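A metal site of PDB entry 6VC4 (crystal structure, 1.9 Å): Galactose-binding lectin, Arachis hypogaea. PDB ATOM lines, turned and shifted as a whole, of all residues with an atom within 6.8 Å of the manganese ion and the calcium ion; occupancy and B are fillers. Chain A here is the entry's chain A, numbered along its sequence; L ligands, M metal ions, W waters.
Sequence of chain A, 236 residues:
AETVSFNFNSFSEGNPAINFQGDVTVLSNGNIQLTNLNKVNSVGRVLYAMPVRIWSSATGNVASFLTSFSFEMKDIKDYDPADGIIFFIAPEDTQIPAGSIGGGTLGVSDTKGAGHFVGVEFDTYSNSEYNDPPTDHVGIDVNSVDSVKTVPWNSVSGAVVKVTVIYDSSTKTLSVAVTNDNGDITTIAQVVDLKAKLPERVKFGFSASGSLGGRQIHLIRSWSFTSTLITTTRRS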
ATOM      1  N   ASP A  83       8.203 -18.123 -25.943  1.00  0.00           N
ATOM      2  CA  ASP A  83       7.012 -17.703 -25.192  1.00  0.00           C
ATOM      3  C   ASP A  83       6.931 -16.214 -24.816  1.00  0.00           C
ATOM      4  O   ASP A  83       5.856 -15.738 -24.461  1.00  0.00           O
ATOM      5  CB  ASP A  83       6.908 -18.526 -23.925  1.00  0.00           C
ATOM      6  CG  ASP A  83       6.231 -19.831 -24.218  1.00  0.00           C
ATOM      7  OD1 ASP A  83       6.953 -20.822 -24.576  1.00  0.00           O
ATOM      8  OD2 ASP A  83       4.995 -19.872 -24.109  1.00  0.00           O
ATOM      9  N   GLY A 103       8.337 -22.580 -21.124  1.00  0.00           N
ATOM     10  CA  GLY A 103       7.036 -22.244 -21.701  1.00  0.00           C
ATOM     11  C   GLY A 103       6.432 -20.946 -21.159  1.00  0.00           C
ATOM     12  O   GLY A 103       7.094 -19.897 -21.129  1.00  0.00           O
ATOM     13  N   GLY A 104       5.194 -21.059 -20.689  1.00  0.00           N
ATOM     14  CA  GLY A 104       4.374 -19.971 -20.146  1.00  0.00           C
ATOM     15  C   GLY A 104       4.823 -19.398 -18.813  1.00  0.00           C
ATOM     16  O   GLY A 104       4.307 -18.363 -18.384  1.00  0.00           O
ATOM     17  N   THR A 105       5.722 -20.123 -18.103  1.00  0.00           N
ATOM     18  CA  THR A 105       6.265 -19.719 -16.795  1.00  0.00           C
ATOM     19  C   THR A 105       7.235 -18.541 -16.958  1.00  0.00           C
ATOM     20  O   THR A 105       7.605 -17.932 -15.959  1.00  0.00           O
ATOM     21  CB  THR A 105       6.970 -20.926 -16.080  1.00  0.00           C
ATOM     22  OG1 THR A 105       8.267 -21.199 -16.657  1.00  0.00           O
ATOM     23  CG2 THR A 105       6.097 -22.165 -16.029  1.00  0.00           C
ATOM     24  N   LEU A 106       7.720 -18.321 -18.204  1.00  0.00           N
ATOM     25  CA  LEU A 106       8.652 -17.276 -18.649  1.00  0.00           C
ATOM     26  C   LEU A 106       9.982 -17.318 -17.862  1.00  0.00           C
ATOM     27  O   LEU A 106      10.741 -16.331 -17.854  1.00  0.00           O
ATOM     28  CB  LEU A 106       8.006 -15.870 -18.578  1.00  0.00           C
ATOM     29  CG  LEU A 106       6.736 -15.645 -19.412  1.00  0.00           C
ATOM     30  CD1 LEU A 106       6.132 -14.248 -19.089  1.00  0.00           C
ATOM     31  CD2 LEU A 106       7.001 -15.810 -20.926  1.00  0.00           C
ATOM     32  N   GLU A 121       5.909  -8.339 -18.444  1.00  0.00           N
ATOM     33  CA  GLU A 121       6.049  -9.387 -19.457  1.00  0.00           C
ATOM     34  C   GLU A 121       5.558  -8.916 -20.827  1.00  0.00           C
ATOM     35  O   GLU A 121       4.597  -8.133 -20.951  1.00  0.00           O
ATOM     36  CB  GLU A 121       5.299 -10.657 -19.041  1.00  0.00           C
ATOM     37  CG  GLU A 121       3.826 -10.401 -18.773  1.00  0.00           C
ATOM     38  CD  GLU A 121       2.947 -11.627 -18.830  1.00  0.00           C
ATOM     39  OE1 GLU A 121       3.112 -12.497 -17.960  1.00  0.00           O
ATOM     40  OE2 GLU A 121       2.048 -11.675 -19.698  1.00  0.00           O
ATOM     41  N   PHE A 122       6.263  -9.389 -21.852  1.00  0.00           N
ATOM     42  CA  PHE A 122       6.035  -9.194 -23.290  1.00  0.00           C
ATOM     43  C   PHE A 122       5.725 -10.609 -23.823  1.00  0.00           C
ATOM     44  O   PHE A 122       6.592 -11.311 -24.325  1.00  0.00           O
ATOM     45  CB  PHE A 122       7.282  -8.518 -23.922  1.00  0.00           C
ATOM     46  CG  PHE A 122       7.594  -7.204 -23.248  1.00  0.00           C
ATOM     47  CD1 PHE A 122       7.003  -6.026 -23.677  1.00  0.00           C
ATOM     48  CD2 PHE A 122       8.438  -7.160 -22.144  1.00  0.00           C
ATOM     49  CE1 PHE A 122       7.259  -4.820 -23.016  1.00  0.00           C
ATOM     50  CE2 PHE A 122       8.682  -5.943 -21.478  1.00  0.00           C
ATOM     51  CZ  PHE A 122       8.077  -4.796 -21.914  1.00  0.00           C
ATOM     52  N   ASP A 123       4.490 -11.030 -23.588  1.00  0.00           N
ATOM     53  CA  ASP A 123       3.977 -12.367 -23.795  1.00  0.00           C
ATOM     54  C   ASP A 123       3.431 -12.641 -25.192  1.00  0.00           C
ATOM     55  O   ASP A 123       2.413 -12.071 -25.579  1.00  0.00           O
ATOM     56  CB  ASP A 123       2.890 -12.602 -22.744  1.00  0.00           C
ATOM     57  CG  ASP A 123       2.549 -14.067 -22.580  1.00  0.00           C
ATOM     58  OD1 ASP A 123       3.012 -14.878 -23.404  1.00  0.00           O
ATOM     59  OD2 ASP A 123       1.898 -14.403 -21.592  1.00  0.00           O
ATOM     60  N   THR A 124       4.047 -13.630 -25.912  1.00  0.00           N
ATOM     61  CA  THR A 124       3.695 -13.963 -27.297  1.00  0.00           C
ATOM     62  C   THR A 124       2.942 -15.290 -27.492  1.00  0.00           C
ATOM     63  O   THR A 124       2.819 -15.754 -28.638  1.00  0.00           O
ATOM     64  CB  THR A 124       4.968 -13.954 -28.152  1.00  0.00           C
ATOM     65  OG1 THR A 124       5.728 -15.147 -27.925  1.00  0.00           O
ATOM     66  CG2 THR A 124       5.822 -12.712 -27.913  1.00  0.00           C
ATOM     67  N   TYR A 125       2.371 -15.851 -26.422  1.00  0.00           N
ATOM     68  CA  TYR A 125       1.616 -17.123 -26.509  1.00  0.00           C
ATOM     69  C   TYR A 125       0.565 -17.159 -25.413  1.00  0.00           C
ATOM     70  O   TYR A 125       0.890 -16.933 -24.243  1.00  0.00           O
ATOM     71  CB  TYR A 125       2.537 -18.374 -26.452  1.00  0.00           C
ATOM     72  CG  TYR A 125       1.739 -19.662 -26.588  1.00  0.00           C
ATOM     73  CD1 TYR A 125       1.443 -20.190 -27.840  1.00  0.00           C
ATOM     74  CD2 TYR A 125       1.165 -20.270 -25.472  1.00  0.00           C
ATOM     75  CE1 TYR A 125       0.619 -21.300 -27.977  1.00  0.00           C
ATOM     76  CE2 TYR A 125       0.287 -21.334 -25.600  1.00  0.00           C
ATOM     77  CZ  TYR A 125       0.048 -21.879 -26.853  1.00  0.00           C
ATOM     78  OH  TYR A 125      -0.757 -22.980 -26.984  1.00  0.00           O
ATOM     79  N   SER A 126      -0.678 -17.466 -25.797  1.00  0.00           N
ATOM     80  CA  SER A 126      -1.814 -17.496 -24.884  1.00  0.00           C
ATOM     81  C   SER A 126      -1.932 -18.837 -24.117  1.00  0.00           C
ATOM     82  O   SER A 126      -2.430 -19.825 -24.657  1.00  0.00           O
ATOM     83  CB  SER A 126      -3.109 -17.181 -25.641  1.00  0.00           C
ATOM     84  OG  SER A 126      -4.199 -17.040 -24.746  1.00  0.00           O
ATOM     85  N   ASN A 127      -1.475 -18.835 -22.853  1.00  0.00           N
ATOM     86  CA  ASN A 127      -1.561 -19.947 -21.910  1.00  0.00           C
ATOM     87  C   ASN A 127      -2.864 -19.866 -21.112  1.00  0.00           C
ATOM     88  O   ASN A 127      -2.945 -19.108 -20.153  1.00  0.00           O
ATOM     89  CB  ASN A 127      -0.355 -19.958 -20.962  1.00  0.00           C
ATOM     90  CG  ASN A 127       0.948 -20.219 -21.634  1.00  0.00           C
ATOM     91  OD1 ASN A 127       1.641 -19.293 -22.068  1.00  0.00           O
ATOM     92  ND2 ASN A 127       1.336 -21.481 -21.716  1.00  0.00           N
ATOM     93  N   TYR A 130      -2.774 -19.974 -17.322  1.00  0.00           N
ATOM     94  CA  TYR A 130      -2.375 -18.768 -16.592  1.00  0.00           C
ATOM     95  C   TYR A 130      -3.332 -17.604 -16.886  1.00  0.00           C
ATOM     96  O   TYR A 130      -3.013 -16.453 -16.623  1.00  0.00           O
ATOM     97  CB  TYR A 130      -0.917 -18.394 -16.899  1.00  0.00           C
ATOM     98  CG  TYR A 130       0.047 -19.542 -16.691  1.00  0.00           C
ATOM     99  CD1 TYR A 130       0.037 -20.289 -15.516  1.00  0.00           C
ATOM    100  CD2 TYR A 130       1.008 -19.851 -17.648  1.00  0.00           C
ATOM    101  CE1 TYR A 130       0.905 -21.360 -15.326  1.00  0.00           C
ATOM    102  CE2 TYR A 130       1.883 -20.920 -17.482  1.00  0.00           C
ATOM    103  CZ  TYR A 130       1.829 -21.660 -16.312  1.00  0.00           C
ATOM    104  OH  TYR A 130       2.707 -22.691 -16.119  1.00  0.00           O
ATOM    105  N   ASN A 131      -4.535 -17.932 -17.427  1.00  0.00           N
ATOM    106  CA  ASN A 131      -5.614 -17.008 -17.793  1.00  0.00           C
ATOM    107  C   ASN A 131      -5.114 -15.879 -18.714  1.00  0.00           C
ATOM    108  O   ASN A 131      -5.526 -14.736 -18.573  1.00  0.00           O
ATOM    109  CB  ASN A 131      -6.317 -16.439 -16.536  1.00  0.00           C
ATOM    110  CG  ASN A 131      -7.098 -17.479 -15.766  1.00  0.00           C
ATOM    111  OD1 ASN A 131      -8.001 -18.149 -16.296  1.00  0.00           O
ATOM    112  ND2 ASN A 131      -6.760 -17.648 -14.486  1.00  0.00           N
ATOM    113  N   ASP A 132      -4.224 -16.230 -19.663  1.00  0.00           N
ATOM    114  CA  ASP A 132      -3.683 -15.275 -20.630  1.00  0.00           C
ATOM    115  C   ASP A 132      -4.792 -14.702 -21.525  1.00  0.00           C
ATOM    116  O   ASP A 132      -5.654 -15.482 -21.953  1.00  0.00           O
ATOM    117  CB  ASP A 132      -2.650 -15.949 -21.524  1.00  0.00           C
ATOM    118  CG  ASP A 132      -1.213 -15.859 -21.049  1.00  0.00           C
ATOM    119  OD1 ASP A 132      -0.913 -14.985 -20.219  1.00  0.00           O
ATOM    120  OD2 ASP A 132      -0.366 -16.616 -21.579  1.00  0.00           O
ATOM    121  N   PRO A 133      -4.730 -13.415 -21.907  1.00  0.00           N
ATOM    122  CA  PRO A 133      -5.717 -12.902 -22.881  1.00  0.00           C
ATOM    123  C   PRO A 133      -5.523 -13.600 -24.250  1.00  0.00           C
ATOM    124  O   PRO A 133      -4.475 -14.256 -24.436  1.00  0.00           O
ATOM    125  CB  PRO A 133      -5.448 -11.383 -22.917  1.00  0.00           C
ATOM    126  CG  PRO A 133      -4.090 -11.203 -22.377  1.00  0.00           C
ATOM    127  CD  PRO A 133      -3.764 -12.363 -21.491  1.00  0.00           C
ATOM    128  N   HIS A 137       0.472  -9.725 -25.640  1.00  0.00           N
ATOM    129  CA  HIS A 137       0.170  -8.701 -24.639  1.00  0.00           C
ATOM    130  C   HIS A 137       1.331  -8.335 -23.748  1.00  0.00           C
ATOM    131  O   HIS A 137       2.267  -9.107 -23.541  1.00  0.00           O
ATOM    132  CB  HIS A 137      -1.007  -9.176 -23.749  1.00  0.00           C
ATOM    133  CG  HIS A 137      -0.757 -10.497 -23.085  1.00  0.00           C
ATOM    134  ND1 HIS A 137      -0.860 -11.709 -23.785  1.00  0.00           N
ATOM    135  CD2 HIS A 137      -0.384 -10.763 -21.811  1.00  0.00           C
ATOM    136  CE1 HIS A 137      -0.591 -12.656 -22.907  1.00  0.00           C
ATOM    137  NE2 HIS A 137      -0.278 -12.142 -21.715  1.00  0.00           N
ATOM    138  N   VAL A 138       1.215  -7.139 -23.168  1.00  0.00           N
ATOM    139  CA  VAL A 138       2.139  -6.652 -22.164  1.00  0.00           C
ATOM    140  C   VAL A 138       1.387  -6.822 -20.859  1.00  0.00           C
ATOM    141  O   VAL A 138       0.204  -6.497 -20.800  1.00  0.00           O
ATOM    142  CB  VAL A 138       2.644  -5.216 -22.422  1.00  0.00           C
ATOM    143  CG1 VAL A 138       3.636  -4.795 -21.339  1.00  0.00           C
ATOM    144  CG2 VAL A 138       3.283  -5.084 -23.800  1.00  0.00           C
ATOM    145  N   GLY A 139       2.030  -7.408 -19.877  1.00  0.00           N
ATOM    146  CA  GLY A 139       1.398  -7.644 -18.592  1.00  0.00           C
ATOM    147  C   GLY A 139       2.228  -7.136 -17.443  1.00  0.00           C
ATOM    148  O   GLY A 139       3.451  -7.015 -17.570  1.00  0.00           O
ATOM    149  N   ASP A 141       2.988  -8.196 -13.650  1.00  0.00           N
ATOM    150  CA  ASP A 141       2.963  -9.452 -12.868  1.00  0.00           C
ATOM    151  C   ASP A 141       3.430  -9.264 -11.452  1.00  0.00           C
ATOM    152  O   ASP A 141       4.475  -8.665 -11.220  1.00  0.00           O
ATOM    153  CB  ASP A 141       3.880 -10.491 -13.535  1.00  0.00           C
ATOM    154  CG  ASP A 141       3.409 -10.986 -14.885  1.00  0.00           C
ATOM    155  OD1 ASP A 141       2.288 -10.599 -15.316  1.00  0.00           O
ATOM    156  OD2 ASP A 141       4.144 -11.791 -15.506  1.00  0.00           O
ATOM    157  N   VAL A 145       2.458 -15.394 -13.140  1.00  0.00           N
ATOM    158  CA  VAL A 145       2.377 -15.170 -14.590  1.00  0.00           C
ATOM    159  C   VAL A 145       0.887 -15.057 -14.978  1.00  0.00           C
ATOM    160  O   VAL A 145       0.572 -14.804 -16.133  1.00  0.00           O
ATOM    161  CB  VAL A 145       3.194 -16.132 -15.499  1.00  0.00           C
ATOM    162  CG1 VAL A 145       4.693 -15.801 -15.459  1.00  0.00           C
ATOM    163  CG2 VAL A 145       2.954 -17.595 -15.166  1.00  0.00           C
ATOM    164  N   ASP A 146      -0.043 -15.162 -13.979  1.00  0.00           N
ATOM    165  CA  ASP A 146      -1.455 -14.808 -14.130  1.00  0.00           C
ATOM    166  C   ASP A 146      -1.466 -13.310 -13.757  1.00  0.00           C
ATOM    167  O   ASP A 146      -1.537 -12.958 -12.569  1.00  0.00           O
ATOM    168  CB  ASP A 146      -2.383 -15.679 -13.257  1.00  0.00           C
ATOM    169  CG  ASP A 146      -3.892 -15.457 -13.466  1.00  0.00           C
ATOM    170  OD1 ASP A 146      -4.279 -14.413 -14.059  1.00  0.00           O
ATOM    171  OD2 ASP A 146      -4.695 -16.311 -13.004  1.00  0.00           O
ATOM    172  N   SER A 147      -1.246 -12.459 -14.767  1.00  0.00           N
ATOM    173  CA  SER A 147      -1.054 -11.021 -14.662  1.00  0.00           C
ATOM    174  C   SER A 147      -2.154 -10.304 -13.892  1.00  0.00           C
ATOM    175  O   SER A 147      -3.337 -10.588 -14.063  1.00  0.00           O
ATOM    176  CB  SER A 147      -0.944 -10.386 -16.047  1.00  0.00           C
ATOM    177  OG  SER A 147       0.113 -10.934 -16.803  1.00  0.00           O
ATOM    178  N   THR A 150      -3.225  -6.683 -18.013  1.00  0.00           N
ATOM    179  CA  THR A 150      -2.634  -6.818 -19.335  1.00  0.00           C
ATOM    180  C   THR A 150      -3.199  -5.763 -20.273  1.00  0.00           C
ATOM    181  O   THR A 150      -4.274  -5.216 -20.033  1.00  0.00           O
ATOM    182  CB  THR A 150      -2.820  -8.237 -19.976  1.00  0.00           C
ATOM    183  OG1 THR A 150      -4.199  -8.480 -20.216  1.00  0.00           O
ATOM    184  CG2 THR A 150      -2.227  -9.330 -19.153  1.00  0.00           C
HETATM  185  C1  LIG L   1       3.914 -22.609 -25.613  1.00  0.00           C
HETATM  186  C2  LIG L   1       3.352 -22.911 -24.226  1.00  0.00           C
HETATM  187  C3  LIG L   1       3.303 -23.574 -26.627  1.00  0.00           C
HETATM  188  C4  LIG L   1       3.000 -25.298 -25.008  1.00  0.00           C
HETATM  189  C5  LIG L   1       3.501 -24.382 -23.881  1.00  0.00           C
HETATM  190  C6  LIG L   1       3.818 -23.382 -28.038  1.00  0.00           C
HETATM  191  C7  LIG L   1       0.611 -30.368 -26.061  1.00  0.00           C
HETATM  192  C8  LIG L   1       1.926 -30.186 -26.789  1.00  0.00           C
HETATM  193  C9  LIG L   1       0.041 -29.028 -25.573  1.00  0.00           C
HETATM  194  C10 LIG L   1       2.291 -28.048 -25.657  1.00  0.00           C
HETATM  195  C11 LIG L   1       2.892 -29.437 -25.894  1.00  0.00           C
HETATM  196  O1  LIG L   1       3.591 -24.925 -26.250  1.00  0.00           O
HETATM  197  O2  LIG L   1       2.827 -24.693 -22.671  1.00  0.00           O
HETATM  198  O3  LIG L   1       4.018 -22.130 -23.241  1.00  0.00           O
HETATM  199  O4  LIG L   1       5.345 -22.703 -25.605  1.00  0.00           O
HETATM  200  O5  LIG L   1       2.920 -23.881 -29.035  1.00  0.00           O
HETATM  201  O6  LIG L   1       1.037 -28.167 -24.981  1.00  0.00           O
HETATM  202  O7  LIG L   1       4.193 -29.367 -26.465  1.00  0.00           O
HETATM  203  O8  LIG L   1       2.484 -31.457 -27.132  1.00  0.00           O
HETATM  204  O9  LIG L   1      -0.309 -31.041 -26.926  1.00  0.00           O
HETATM  205  S1  LIG L   1       3.394 -27.018 -24.644  1.00  0.00           S
HETATM  206 MN    MN M   1       0.625 -13.324 -20.303  1.00  0.00          MN
HETATM  207 CA    CA M   2       1.877 -16.801 -22.239  1.00  0.00          CA
HETATM  208  O   HOH W   1       1.700 -14.657 -18.474  1.00  0.00           O
HETATM  209  O   HOH W   2       3.826 -17.427 -23.117  1.00  0.00           O
HETATM  210  O   HOH W   3       2.580 -16.973 -19.873  1.00  0.00           O
HETATM  211  O   HOH W   4      -0.856 -12.360 -18.925  1.00  0.00           O
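Four residues have an atom within 4 Å of the calcium ion: Asp 123, Tyr 125, Asn 127 and Asp 132.
The manganese ion is bound by a ring nitrogen (NE2) of His 137 (2.1 Å), the side-chain carboxylate (OD2) of Asp 123 (2.1 Å), water W4 (2.2 Å), the side-chain carboxylate (OE2) of Glu 121 (2.3 Å), the side-chain carboxylate (OD1) of Asp 132 (2.3 Å) and water W1 (2.5 Å).
Water W1 lies within hydrogen-bond range of O of Val 145 and OE1 of Glu 121.
Four residues have an atom within 4 Å of the manganese ion: Glu 121, Asp 123, Asp 132 and His 137.
The side-chain amide nitrogen (ND2) of Asn 127 lies within hydrogen-bond range of an oxygen (O3) of the ligand (3.2 Å). The backbone NH (N) of Gly 104 sits at hydrogen-bond distance from an oxygen (O3) of the ligand, 3.0 Å away. The side-chain carboxylate (OD2) of Asp 83 sits at hydrogen-bond distance from an oxygen (O3) of the ligand (2.6 Å).
Water W2 binds the calcium ion (2.2 Å). O of Tyr 125 is bound to the calcium ion (2.2 Å). The calcium ion is bound by OD2 of Asp 132 (2.3 Å). Water W3 is bound to the calcium ion (2.5 Å). The side-chain carboxylate (OD2) of Asp 123 binds the calcium ion. The calcium ion is bound by OD1 of Asn 127 (2.5 Å). The side-chain carboxylate (OD1) of Asp 123 is bound to the calcium ion (2.5 Å). The calcium ion has seven donor atoms within binding distance.
O of Glu 121 is in hydrogen-bond range of N of Gly 139 (2.9 Å).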
